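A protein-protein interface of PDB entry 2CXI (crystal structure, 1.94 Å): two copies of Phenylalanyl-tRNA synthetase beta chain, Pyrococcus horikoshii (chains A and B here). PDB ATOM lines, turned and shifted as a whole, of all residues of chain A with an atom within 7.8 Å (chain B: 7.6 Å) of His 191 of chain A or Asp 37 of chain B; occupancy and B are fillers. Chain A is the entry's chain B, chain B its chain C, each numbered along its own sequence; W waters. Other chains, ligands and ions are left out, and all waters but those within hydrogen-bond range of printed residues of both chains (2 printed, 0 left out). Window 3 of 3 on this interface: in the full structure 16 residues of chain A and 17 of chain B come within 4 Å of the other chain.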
ATOM      1  N   ARG A 135     -21.240 -28.522   2.707  1.00  0.00           N
ATOM      2  CA  ARG A 135     -21.414 -27.186   3.317  1.00  0.00           C
ATOM      3  C   ARG A 135     -22.889 -26.754   3.175  1.00  0.00           C
ATOM      4  O   ARG A 135     -23.179 -25.780   2.512  1.00  0.00           O
ATOM      5  CB  ARG A 135     -20.508 -26.182   2.582  1.00  0.00           C
ATOM      6  CG  ARG A 135     -19.944 -25.038   3.434  1.00  0.00           C
ATOM      7  CD  ARG A 135     -18.466 -25.237   3.852  1.00  0.00           C
ATOM      8  NE  ARG A 135     -18.234 -25.627   5.253  1.00  0.00           N
ATOM      9  CZ  ARG A 135     -18.147 -24.783   6.299  1.00  0.00           C
ATOM     10  NH1 ARG A 135     -17.898 -25.236   7.512  1.00  0.00           N
ATOM     11  NH2 ARG A 135     -18.329 -23.493   6.148  1.00  0.00           N
ATOM     12  N   ARG A 136     -23.802 -27.530   3.737  1.00  0.00           N
ATOM     13  CA  ARG A 136     -25.240 -27.262   3.652  1.00  0.00           C
ATOM     14  C   ARG A 136     -25.684 -27.014   2.206  1.00  0.00           C
ATOM     15  O   ARG A 136     -26.283 -25.968   1.881  1.00  0.00           O
ATOM     16  CB  ARG A 136     -25.633 -26.104   4.595  1.00  0.00           C
ATOM     17  CG  ARG A 136     -25.157 -26.318   6.036  1.00  0.00           C
ATOM     18  CD  ARG A 136     -25.508 -25.195   7.020  1.00  0.00           C
ATOM     19  NE  ARG A 136     -24.581 -24.058   6.870  1.00  0.00           N
ATOM     20  CZ  ARG A 136     -24.878 -22.916   6.270  1.00  0.00           C
ATOM     21  NH1 ARG A 136     -26.088 -22.731   5.751  1.00  0.00           N
ATOM     22  NH2 ARG A 136     -23.972 -21.946   6.197  1.00  0.00           N
ATOM     23  N   ARG A 138     -24.373 -25.924  -0.490  1.00  0.00           N
ATOM     24  CA  ARG A 138     -23.810 -24.943  -1.419  1.00  0.00           C
ATOM     25  C   ARG A 138     -22.768 -25.584  -2.341  1.00  0.00           C
ATOM     26  O   ARG A 138     -22.800 -25.402  -3.556  1.00  0.00           O
ATOM     27  CB  ARG A 138     -23.199 -23.728  -0.705  1.00  0.00           C
ATOM     28  CG  ARG A 138     -23.167 -22.533  -1.656  1.00  0.00           C
ATOM     29  CD  ARG A 138     -22.429 -21.258  -1.144  1.00  0.00           C
ATOM     30  NE  ARG A 138     -21.125 -21.301  -1.750  1.00  0.00           N
ATOM     31  CZ  ARG A 138     -20.094 -21.914  -1.195  1.00  0.00           C
ATOM     32  NH1 ARG A 138     -18.997 -21.959  -1.884  1.00  0.00           N
ATOM     33  NH2 ARG A 138     -20.164 -22.458   0.053  1.00  0.00           N
ATOM     34  N   LEU A 180     -39.222 -20.968  -4.266  1.00  0.00           N
ATOM     35  CA  LEU A 180     -38.222 -20.340  -3.399  1.00  0.00           C
ATOM     36  C   LEU A 180     -38.895 -19.543  -2.313  1.00  0.00           C
ATOM     37  O   LEU A 180     -38.386 -19.456  -1.198  1.00  0.00           O
ATOM     38  CB  LEU A 180     -37.310 -19.416  -4.196  1.00  0.00           C
ATOM     39  CG  LEU A 180     -36.345 -20.019  -5.226  1.00  0.00           C
ATOM     40  CD1 LEU A 180     -35.259 -19.003  -5.588  1.00  0.00           C
ATOM     41  CD2 LEU A 180     -35.718 -21.314  -4.724  1.00  0.00           C
ATOM     42  N   LYS A 185     -37.944 -25.662   1.588  1.00  0.00           N
ATOM     43  CA  LYS A 185     -36.571 -25.760   1.095  1.00  0.00           C
ATOM     44  C   LYS A 185     -36.158 -24.545   0.278  1.00  0.00           C
ATOM     45  O   LYS A 185     -34.962 -24.186   0.212  1.00  0.00           O
ATOM     46  CB  LYS A 185     -36.399 -27.067   0.303  1.00  0.00           C
ATOM     47  CG  LYS A 185     -36.663 -28.300   1.142  1.00  0.00           C
ATOM     48  CD  LYS A 185     -35.639 -28.481   2.261  1.00  0.00           C
ATOM     49  CE  LYS A 185     -36.012 -29.684   3.121  1.00  0.00           C
ATOM     50  NZ  LYS A 185     -34.974 -29.930   4.163  1.00  0.00           N
ATOM     51  N   GLY A 186     -37.147 -23.908  -0.350  1.00  0.00           N
ATOM     52  CA  GLY A 186     -36.927 -22.627  -1.017  1.00  0.00           C
ATOM     53  C   GLY A 186     -36.494 -21.556  -0.016  1.00  0.00           C
ATOM     54  O   GLY A 186     -35.519 -20.843  -0.244  1.00  0.00           O
ATOM     55  N   ARG A 187     -37.233 -21.437   1.087  1.00  0.00           N
ATOM     56  CA  ARG A 187     -36.888 -20.495   2.147  1.00  0.00           C
ATOM     57  C   ARG A 187     -35.485 -20.769   2.692  1.00  0.00           C
ATOM     58  O   ARG A 187     -34.683 -19.847   2.852  1.00  0.00           O
ATOM     59  CB  ARG A 187     -37.917 -20.567   3.276  1.00  0.00           C
ATOM     60  CG  ARG A 187     -39.225 -19.794   2.933  1.00  0.00           C
ATOM     61  CD  ARG A 187     -40.251 -19.750   4.054  1.00  0.00           C
ATOM     62  NE  ARG A 187     -41.343 -20.685   3.790  1.00  0.00           N
ATOM     63  CZ  ARG A 187     -41.572 -21.795   4.491  1.00  0.00           C
ATOM     64  NH1 ARG A 187     -40.802 -22.106   5.537  1.00  0.00           N
ATOM     65  NH2 ARG A 187     -42.571 -22.598   4.137  1.00  0.00           N
ATOM     66  N   GLU A 188     -35.207 -22.047   2.935  1.00  0.00           N
ATOM     67  CA  GLU A 188     -33.943 -22.484   3.531  1.00  0.00           C
ATOM     68  C   GLU A 188     -32.718 -22.299   2.626  1.00  0.00           C
ATOM     69  O   GLU A 188     -31.688 -21.764   3.063  1.00  0.00           O
ATOM     70  CB  GLU A 188     -34.060 -23.933   4.009  1.00  0.00           C
ATOM     71  CG  GLU A 188     -32.898 -24.400   4.874  1.00  0.00           C
ATOM     72  CD  GLU A 188     -33.037 -25.846   5.327  1.00  0.00           C
ATOM     73  OE1 GLU A 188     -34.099 -26.468   5.087  1.00  0.00           O
ATOM     74  OE2 GLU A 188     -32.066 -26.374   5.919  1.00  0.00           O
ATOM     75  N   TYR A 189     -32.831 -22.721   1.360  1.00  0.00           N
ATOM     76  CA  TYR A 189     -31.685 -22.744   0.475  1.00  0.00           C
ATOM     77  C   TYR A 189     -31.759 -21.755  -0.668  1.00  0.00           C
ATOM     78  O   TYR A 189     -30.784 -21.609  -1.407  1.00  0.00           O
ATOM     79  CB  TYR A 189     -31.498 -24.151  -0.075  1.00  0.00           C
ATOM     80  CG  TYR A 189     -31.162 -25.185   0.950  1.00  0.00           C
ATOM     81  CD1 TYR A 189     -29.897 -25.229   1.529  1.00  0.00           C
ATOM     82  CD2 TYR A 189     -32.101 -26.138   1.332  1.00  0.00           C
ATOM     83  CE1 TYR A 189     -29.574 -26.200   2.454  1.00  0.00           C
ATOM     84  CE2 TYR A 189     -31.796 -27.103   2.267  1.00  0.00           C
ATOM     85  CZ  TYR A 189     -30.523 -27.130   2.813  1.00  0.00           C
ATOM     86  OH  TYR A 189     -30.215 -28.080   3.731  1.00  0.00           O
ATOM     87  N   GLY A 190     -32.904 -21.077  -0.838  1.00  0.00           N
ATOM     88  CA  GLY A 190     -33.074 -20.161  -1.965  1.00  0.00           C
ATOM     89  C   GLY A 190     -32.016 -19.066  -2.119  1.00  0.00           C
ATOM     90  O   GLY A 190     -31.733 -18.612  -3.237  1.00  0.00           O
ATOM     91  N   HIS A 191     -31.420 -18.622  -1.021  1.00  0.00           N
ATOM     92  CA  HIS A 191     -30.476 -17.482  -1.114  1.00  0.00           C
ATOM     93  C   HIS A 191     -29.278 -17.806  -2.032  1.00  0.00           C
ATOM     94  O   HIS A 191     -28.671 -16.903  -2.646  1.00  0.00           O
ATOM     95  CB  HIS A 191     -29.978 -17.046   0.270  1.00  0.00           C
ATOM     96  CG  HIS A 191     -29.142 -18.076   0.974  1.00  0.00           C
ATOM     97  ND1 HIS A 191     -27.757 -18.068   0.938  1.00  0.00           N
ATOM     98  CD2 HIS A 191     -29.491 -19.141   1.734  1.00  0.00           C
ATOM     99  CE1 HIS A 191     -27.297 -19.088   1.642  1.00  0.00           C
ATOM    100  NE2 HIS A 191     -28.327 -19.758   2.134  1.00  0.00           N
ATOM    101  N   LEU A 192     -28.984 -19.108  -2.152  1.00  0.00           N
ATOM    102  CA  LEU A 192     -27.913 -19.617  -2.992  1.00  0.00           C
ATOM    103  C   LEU A 192     -28.087 -19.291  -4.456  1.00  0.00           C
ATOM    104  O   LEU A 192     -27.105 -19.207  -5.181  1.00  0.00           O
ATOM    105  CB  LEU A 192     -27.799 -21.130  -2.830  1.00  0.00           C
ATOM    106  CG  LEU A 192     -27.491 -21.586  -1.418  1.00  0.00           C
ATOM    107  CD1 LEU A 192     -27.487 -23.082  -1.387  1.00  0.00           C
ATOM    108  CD2 LEU A 192     -26.135 -21.027  -1.014  1.00  0.00           C
ATOM    109  N   ILE A 193     -29.327 -19.075  -4.886  1.00  0.00           N
ATOM    110  CA  ILE A 193     -29.587 -18.795  -6.296  1.00  0.00           C
ATOM    111  C   ILE A 193     -30.515 -17.610  -6.578  1.00  0.00           C
ATOM    112  O   ILE A 193     -30.629 -17.188  -7.735  1.00  0.00           O
ATOM    113  CB  ILE A 193     -30.146 -20.077  -7.019  1.00  0.00           C
ATOM    114  CG1 ILE A 193     -31.399 -20.593  -6.321  1.00  0.00           C
ATOM    115  CG2 ILE A 193     -29.088 -21.240  -7.032  1.00  0.00           C
ATOM    116  CD1 ILE A 193     -32.147 -21.592  -7.138  1.00  0.00           C
ATOM    117  N   LYS A 194     -31.201 -17.111  -5.557  1.00  0.00           N
ATOM    118  CA  LYS A 194     -32.330 -16.166  -5.786  1.00  0.00           C
ATOM    119  C   LYS A 194     -31.925 -14.860  -6.490  1.00  0.00           C
ATOM    120  O   LYS A 194     -32.715 -14.270  -7.234  1.00  0.00           O
ATOM    121  CB  LYS A 194     -33.100 -15.874  -4.492  1.00  0.00           C
ATOM    122  CG  LYS A 194     -32.406 -14.882  -3.570  1.00  0.00           C
ATOM    123  CD  LYS A 194     -33.077 -14.836  -2.216  1.00  0.00           C
ATOM    124  CE  LYS A 194     -32.448 -13.744  -1.336  1.00  0.00           C
ATOM    125  NZ  LYS A 194     -33.114 -13.646   0.002  1.00  0.00           N
ATOM    126  N   ASP A 195     -30.681 -14.442  -6.314  1.00  0.00           N
ATOM    127  CA  ASP A 195     -30.248 -13.184  -6.915  1.00  0.00           C
ATOM    128  C   ASP A 195     -29.730 -13.288  -8.354  1.00  0.00           C
ATOM    129  O   ASP A 195     -29.278 -12.285  -8.943  1.00  0.00           O
ATOM    130  CB  ASP A 195     -29.272 -12.457  -5.971  1.00  0.00           C
ATOM    131  CG  ASP A 195     -29.969 -11.988  -4.679  1.00  0.00           C
ATOM    132  OD1 ASP A 195     -30.933 -11.214  -4.795  1.00  0.00           O
ATOM    133  OD2 ASP A 195     -29.661 -12.362  -3.521  1.00  0.00           O
ATOM    134  N   LYS A 196     -29.807 -14.486  -8.934  1.00  0.00           N
ATOM    135  CA  LYS A 196     -29.311 -14.664 -10.272  1.00  0.00           C
ATOM    136  C   LYS A 196     -30.445 -14.444 -11.273  1.00  0.00           C
ATOM    137  O   LYS A 196     -31.602 -14.474 -10.911  1.00  0.00           O
ATOM    138  CB  LYS A 196     -28.637 -16.043 -10.444  1.00  0.00           C
ATOM    139  CG  LYS A 196     -27.704 -16.458  -9.274  1.00  0.00           C
ATOM    140  CD  LYS A 196     -26.561 -15.500  -8.998  1.00  0.00           C
ATOM    141  CE  LYS A 196     -25.544 -15.497 -10.129  1.00  0.00           C
ATOM    142  NZ  LYS A 196     -24.245 -14.902  -9.729  1.00  0.00           N
ATOM    143  N   ILE A 215     -32.286 -27.030  -4.435  1.00  0.00           N
ATOM    144  CA  ILE A 215     -33.446 -26.699  -3.588  1.00  0.00           C
ATOM    145  C   ILE A 215     -34.366 -27.890  -3.291  1.00  0.00           C
ATOM    146  O   ILE A 215     -34.525 -28.285  -2.139  1.00  0.00           O
ATOM    147  CB  ILE A 215     -34.222 -25.499  -4.194  1.00  0.00           C
ATOM    148  CG1 ILE A 215     -33.273 -24.352  -4.636  1.00  0.00           C
ATOM    149  CG2 ILE A 215     -35.387 -25.055  -3.285  1.00  0.00           C
ATOM    150  CD1 ILE A 215     -32.440 -23.667  -3.538  1.00  0.00           C
ATOM    151  N   PHE B   4     -16.899 -15.460  10.614  1.00  0.00           N
ATOM    152  CA  PHE B   4     -16.995 -14.009  10.517  1.00  0.00           C
ATOM    153  C   PHE B   4     -17.409 -13.631   9.092  1.00  0.00           C
ATOM    154  O   PHE B   4     -17.134 -14.386   8.165  1.00  0.00           O
ATOM    155  CB  PHE B   4     -15.656 -13.368  10.909  1.00  0.00           C
ATOM    156  CG  PHE B   4     -14.480 -13.816  10.062  1.00  0.00           C
ATOM    157  CD1 PHE B   4     -13.861 -15.048  10.291  1.00  0.00           C
ATOM    158  CD2 PHE B   4     -13.968 -12.974   9.053  1.00  0.00           C
ATOM    159  CE1 PHE B   4     -12.753 -15.463   9.524  1.00  0.00           C
ATOM    160  CE2 PHE B   4     -12.863 -13.371   8.267  1.00  0.00           C
ATOM    161  CZ  PHE B   4     -12.267 -14.637   8.499  1.00  0.00           C
ATOM    162  N   ASP B   5     -18.072 -12.483   8.926  1.00  0.00           N
ATOM    163  CA  ASP B   5     -18.527 -12.050   7.604  1.00  0.00           C
ATOM    164  C   ASP B   5     -17.584 -11.069   6.992  1.00  0.00           C
ATOM    165  O   ASP B   5     -16.954 -10.251   7.695  1.00  0.00           O
ATOM    166  CB  ASP B   5     -19.902 -11.357   7.662  1.00  0.00           C
ATOM    167  CG  ASP B   5     -20.968 -12.228   8.233  1.00  0.00           C
ATOM    168  OD1 ASP B   5     -20.845 -13.481   8.270  1.00  0.00           O
ATOM    169  OD2 ASP B   5     -21.998 -11.720   8.665  1.00  0.00           O
ATOM    170  N   VAL B   6     -17.513 -11.098   5.661  1.00  0.00           N
ATOM    171  CA  VAL B   6     -16.628 -10.176   4.953  1.00  0.00           C
ATOM    172  C   VAL B   6     -17.344  -9.796   3.674  1.00  0.00           C
ATOM    173  O   VAL B   6     -18.220 -10.517   3.219  1.00  0.00           O
ATOM    174  CB  VAL B   6     -15.282 -10.844   4.576  1.00  0.00           C
ATOM    175  CG1 VAL B   6     -14.364 -11.028   5.811  1.00  0.00           C
ATOM    176  CG2 VAL B   6     -15.536 -12.205   3.899  1.00  0.00           C
ATOM    177  N   GLU B  34     -12.843 -21.819   5.486  1.00  0.00           N
ATOM    178  CA  GLU B  34     -13.822 -22.400   4.574  1.00  0.00           C
ATOM    179  C   GLU B  34     -14.891 -21.358   4.242  1.00  0.00           C
ATOM    180  O   GLU B  34     -15.202 -20.482   5.067  1.00  0.00           O
ATOM    181  CB  GLU B  34     -14.521 -23.627   5.200  1.00  0.00           C
ATOM    182  CG  GLU B  34     -13.627 -24.773   5.638  1.00  0.00           C
ATOM    183  CD  GLU B  34     -12.861 -25.420   4.502  1.00  0.00           C
ATOM    184  OE1 GLU B  34     -12.648 -26.649   4.563  1.00  0.00           O
ATOM    185  OE2 GLU B  34     -12.430 -24.709   3.556  1.00  0.00           O
ATOM    186  N   LEU B  35     -15.487 -21.489   3.060  1.00  0.00           N
ATOM    187  CA  LEU B  35     -16.545 -20.582   2.653  1.00  0.00           C
ATOM    188  C   LEU B  35     -17.843 -21.115   3.187  1.00  0.00           C
ATOM    189  O   LEU B  35     -18.402 -22.075   2.623  1.00  0.00           O
ATOM    190  CB  LEU B  35     -16.645 -20.534   1.140  1.00  0.00           C
ATOM    191  CG  LEU B  35     -16.759 -19.190   0.467  1.00  0.00           C
ATOM    192  CD1 LEU B  35     -17.095 -19.388  -1.009  1.00  0.00           C
ATOM    193  CD2 LEU B  35     -17.685 -18.214   1.174  1.00  0.00           C
ATOM    194  N   ASP B  36     -18.330 -20.512   4.262  1.00  0.00           N
ATOM    195  CA  ASP B  36     -19.434 -21.110   4.986  1.00  0.00           C
ATOM    196  C   ASP B  36     -20.728 -20.767   4.296  1.00  0.00           C
ATOM    197  O   ASP B  36     -21.656 -21.594   4.248  1.00  0.00           O
ATOM    198  CB  ASP B  36     -19.476 -20.648   6.453  1.00  0.00           C
ATOM    199  CG  ASP B  36     -20.497 -21.427   7.266  1.00  0.00           C
ATOM    200  OD1 ASP B  36     -20.330 -22.650   7.435  1.00  0.00           O
ATOM    201  OD2 ASP B  36     -21.513 -20.916   7.752  1.00  0.00           O
ATOM    202  N   ASP B  37     -20.789 -19.541   3.766  1.00  0.00           N
ATOM    203  CA  ASP B  37     -21.967 -19.071   3.056  1.00  0.00           C
ATOM    204  C   ASP B  37     -21.624 -17.943   2.085  1.00  0.00           C
ATOM    205  O   ASP B  37     -20.590 -17.267   2.228  1.00  0.00           O
ATOM    206  CB  ASP B  37     -23.036 -18.614   4.063  1.00  0.00           C
ATOM    207  CG  ASP B  37     -24.431 -18.680   3.503  1.00  0.00           C
ATOM    208  OD1 ASP B  37     -24.627 -19.193   2.365  1.00  0.00           O
ATOM    209  OD2 ASP B  37     -25.407 -18.196   4.132  1.00  0.00           O
ATOM    210  N   VAL B  38     -22.477 -17.782   1.077  1.00  0.00           N
ATOM    211  CA  VAL B  38     -22.399 -16.688   0.121  1.00  0.00           C
ATOM    212  C   VAL B  38     -23.792 -16.174  -0.086  1.00  0.00           C
ATOM    213  O   VAL B  38     -24.740 -16.956  -0.355  1.00  0.00           O
ATOM    214  CB  VAL B  38     -21.844 -17.116  -1.276  1.00  0.00           C
ATOM    215  CG1 VAL B  38     -21.684 -15.887  -2.195  1.00  0.00           C
ATOM    216  CG2 VAL B  38     -20.521 -17.868  -1.151  1.00  0.00           C
ATOM    217  N   TRP B  39     -23.940 -14.865   0.041  1.00  0.00           N
ATOM    218  CA  TRP B  39     -25.225 -14.258  -0.215  1.00  0.00           C
ATOM    219  C   TRP B  39     -24.980 -12.845  -0.709  1.00  0.00           C
ATOM    220  O   TRP B  39     -23.850 -12.350  -0.697  1.00  0.00           O
ATOM    221  CB  TRP B  39     -26.116 -14.259   1.053  1.00  0.00           C
ATOM    222  CG  TRP B  39     -25.693 -13.241   2.119  1.00  0.00           C
ATOM    223  CD1 TRP B  39     -26.195 -11.959   2.321  1.00  0.00           C
ATOM    224  CD2 TRP B  39     -24.655 -13.413   3.081  1.00  0.00           C
ATOM    225  NE1 TRP B  39     -25.522 -11.348   3.360  1.00  0.00           N
ATOM    226  CE2 TRP B  39     -24.581 -12.222   3.849  1.00  0.00           C
ATOM    227  CE3 TRP B  39     -23.770 -14.464   3.376  1.00  0.00           C
ATOM    228  CZ2 TRP B  39     -23.666 -12.064   4.894  1.00  0.00           C
ATOM    229  CZ3 TRP B  39     -22.878 -14.306   4.423  1.00  0.00           C
ATOM    230  CH2 TRP B  39     -22.826 -13.105   5.160  1.00  0.00           C
ATOM    231  N   GLU B  40     -26.057 -12.209  -1.137  1.00  0.00           N
ATOM    232  CA  GLU B  40     -26.040 -10.869  -1.665  1.00  0.00           C
ATOM    233  C   GLU B  40     -27.030 -10.025  -0.855  1.00  0.00           C
ATOM    234  O   GLU B  40     -28.061 -10.536  -0.374  1.00  0.00           O
ATOM    235  CB  GLU B  40     -26.500 -10.952  -3.114  1.00  0.00           C
ATOM    236  CG  GLU B  40     -25.829 -10.017  -4.071  1.00  0.00           C
ATOM    237  CD  GLU B  40     -26.242 -10.318  -5.494  1.00  0.00           C
ATOM    238  OE1 GLU B  40     -25.772 -11.347  -6.043  1.00  0.00           O
ATOM    239  OE2 GLU B  40     -27.051  -9.537  -6.043  1.00  0.00           O
ATOM    240  N   VAL B  45     -22.035  -8.549  -2.650  1.00  0.00           N
ATOM    241  CA  VAL B  45     -21.806  -9.948  -2.281  1.00  0.00           C
ATOM    242  C   VAL B  45     -21.033 -10.045  -0.951  1.00  0.00           C
ATOM    243  O   VAL B  45     -19.973  -9.409  -0.810  1.00  0.00           O
ATOM    244  CB  VAL B  45     -21.063 -10.724  -3.408  1.00  0.00           C
ATOM    245  CG1 VAL B  45     -20.711 -12.150  -2.960  1.00  0.00           C
ATOM    246  CG2 VAL B  45     -21.935 -10.773  -4.667  1.00  0.00           C
ATOM    247  N   TYR B  46     -21.548 -10.872  -0.030  1.00  0.00           N
ATOM    248  CA  TYR B  46     -20.882 -11.168   1.238  1.00  0.00           C
ATOM    249  C   TYR B  46     -20.559 -12.623   1.373  1.00  0.00           C
ATOM    250  O   TYR B  46     -21.229 -13.478   0.786  1.00  0.00           O
ATOM    251  CB  TYR B  46     -21.741 -10.740   2.433  1.00  0.00           C
ATOM    252  CG  TYR B  46     -21.990  -9.261   2.422  1.00  0.00           C
ATOM    253  CD1 TYR B  46     -21.098  -8.394   3.029  1.00  0.00           C
ATOM    254  CD2 TYR B  46     -23.113  -8.725   1.784  1.00  0.00           C
ATOM    255  CE1 TYR B  46     -21.297  -7.021   2.986  1.00  0.00           C
ATOM    256  CE2 TYR B  46     -23.330  -7.347   1.756  1.00  0.00           C
ATOM    257  CZ  TYR B  46     -22.405  -6.517   2.359  1.00  0.00           C
ATOM    258  OH  TYR B  46     -22.585  -5.161   2.344  1.00  0.00           O
ATOM    259  N   PHE B  47     -19.512 -12.896   2.154  1.00  0.00           N
ATOM    260  CA  PHE B  47     -19.095 -14.254   2.457  1.00  0.00           C
ATOM    261  C   PHE B  47     -19.213 -14.370   3.961  1.00  0.00           C
ATOM    262  O   PHE B  47     -18.907 -13.402   4.679  1.00  0.00           O
ATOM    263  CB  PHE B  47     -17.609 -14.539   2.108  1.00  0.00           C
ATOM    264  CG  PHE B  47     -17.239 -14.387   0.643  1.00  0.00           C
ATOM    265  CD1 PHE B  47     -18.175 -14.612  -0.380  1.00  0.00           C
ATOM    266  CD2 PHE B  47     -15.925 -14.031   0.296  1.00  0.00           C
ATOM    267  CE1 PHE B  47     -17.820 -14.476  -1.737  1.00  0.00           C
ATOM    268  CE2 PHE B  47     -15.539 -13.895  -1.073  1.00  0.00           C
ATOM    269  CZ  PHE B  47     -16.493 -14.112  -2.071  1.00  0.00           C
ATOM    270  N   LYS B  48     -19.658 -15.531   4.426  1.00  0.00           N
ATOM    271  CA  LYS B  48     -19.359 -15.935   5.794  1.00  0.00           C
ATOM    272  C   LYS B  48     -18.199 -16.951   5.761  1.00  0.00           C
ATOM    273  O   LYS B  48     -18.272 -18.012   5.118  1.00  0.00           O
ATOM    274  CB  LYS B  48     -20.576 -16.517   6.511  1.00  0.00           C
ATOM    275  CG  LYS B  48     -20.253 -16.963   7.962  1.00  0.00           C
ATOM    276  CD  LYS B  48     -21.404 -17.695   8.590  1.00  0.00           C
ATOM    277  CE  LYS B  48     -22.701 -16.889   8.600  1.00  0.00           C
ATOM    278  NZ  LYS B  48     -22.525 -15.575   9.294  1.00  0.00           N
ATOM    279  N   LEU B  49     -17.111 -16.615   6.440  1.00  0.00           N
ATOM    280  CA  LEU B  49     -15.925 -17.453   6.400  1.00  0.00           C
ATOM    281  C   LEU B  49     -15.828 -18.165   7.719  1.00  0.00           C
ATOM    282  O   LEU B  49     -16.239 -17.617   8.733  1.00  0.00           O
ATOM    283  CB  LEU B  49     -14.649 -16.619   6.136  1.00  0.00           C
ATOM    284  CG  LEU B  49     -14.626 -15.837   4.811  1.00  0.00           C
ATOM    285  CD1 LEU B  49     -13.257 -15.157   4.658  1.00  0.00           C
ATOM    286  CD2 LEU B  49     -14.899 -16.821   3.612  1.00  0.00           C
ATOM    287  N   ASP B  50     -15.330 -19.392   7.698  1.00  0.00           N
ATOM    288  CA  ASP B  50     -15.192 -20.161   8.919  1.00  0.00           C
ATOM    289  C   ASP B  50     -13.698 -20.465   9.126  1.00  0.00           C
ATOM    290  O   ASP B  50     -13.098 -21.216   8.366  1.00  0.00           O
ATOM    291  CB  ASP B  50     -16.035 -21.448   8.821  1.00  0.00           C
ATOM    292  CG  ASP B  50     -15.909 -22.357  10.073  1.00  0.00           C
ATOM    293  OD1 ASP B  50     -15.319 -21.948  11.089  1.00  0.00           O
ATOM    294  OD2 ASP B  50     -16.378 -23.511  10.108  1.00  0.00           O
HETATM  295  O   HOH W   1     -28.471 -13.972  -1.894  1.00  0.00           O
HETATM  296  O   HOH W   2     -22.655 -22.662   2.266  1.00  0.00           O
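The guanidinium group (NH2) of Arg 135 of chain A is in salt-bridge range of the side-chain carboxylate (OD1) of Asp 36 of chain B.
The guanidinium group (NH1) of Arg 135 of chain A lies within salt-bridge range of the side-chain carboxylate (OD2) of Asp 50 of chain B, at 3.5 Å.
The guanidinium group (NH2) of Arg 136 of chain A lies within salt-bridge range of the side-chain carboxylate (OD2) of Asp 36 of chain B (3.1 Å).
The guanidinium group (NH2) of Arg 138 of chain A sits at hydrogen-bond distance from the backbone carbonyl oxygen (O) of Leu 35 of chain B (3.1 Å).
O of Val 38 of chain B lies within hydrogen-bond range of ND1 of His 191 of chain A, at 3.5 Å.
The backbone NH (N) of Asp 50 of chain B lies within hydrogen-bond range of the backbone carbonyl oxygen (O) of Glu 34 of chain B, 2.9 Å away.
O of Lys 48 of chain B lies within hydrogen-bond range of N of Asp 36 of chain B.
The backbone NH (N) of Lys 48 of chain B is in hydrogen-bond range of the backbone carbonyl oxygen (O) of Asp 37 of chain B (3.0 Å).
Arg 135 of chain A touches Glu 34 of chain B (NH2 to CB, 3.9 Å).
Arg 135 of chain A touches Leu 35 of chain B (CD to O, 3.4 Å).
Val 38 of chain B touches Arg 138 of chain A (CG2 to NE, 3.5 Å).
His 191 of chain A touches Asp 37 of chain B.
Asp 195 of chain A touches Glu 40 of chain B (OD2 to CB, 3.5 Å).
No residue of chain B comes within 4 Å of Gly 190 of chain A.
His 191 of chain A touches just these residues of chain B: Asp 37 (2.8 Å) and Val 38 (3.5 Å).
Printed residues of chain B within 4 Å of Asp 195 of chain A: Glu 40 (3.5 Å).
Of the printed residues of chain A, Asp 50 of chain B touches Arg 135 (3.5 Å).
Of the 16 printed residues of chain B, 7 touch a printed residue of chain A.
Of the 17 printed residues of chain A, 5 touch a printed residue of chain B.
Printed residues of chain A that touch a printed residue of chain B: Arg 135, Arg 136, Arg 138, His 191 and Asp 195.
Hydrophobic or aromatic side chains of chain A within 4 Å of the printed part of chain B: His 191.
No position is printed for both chains.
Of the 10 pairs that touch across the chains among the printed residues, none has its exchanged pair printed and touching as well.
Water W2 lies within hydrogen-bond range of O of Asp 36 of chain B, O of Arg 135 of chain A and NH2 of Arg 138 of chain A.
Water W1 lies within hydrogen-bond range of the side-chain carboxylate (OD2) of Asp 195 of chain A (2.6 Å), the backbone carbonyl oxygen (O) of His 191 of chain A (3.0 Å) and the backbone NH (N) of Glu 40 of chain B (3.1 Å).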
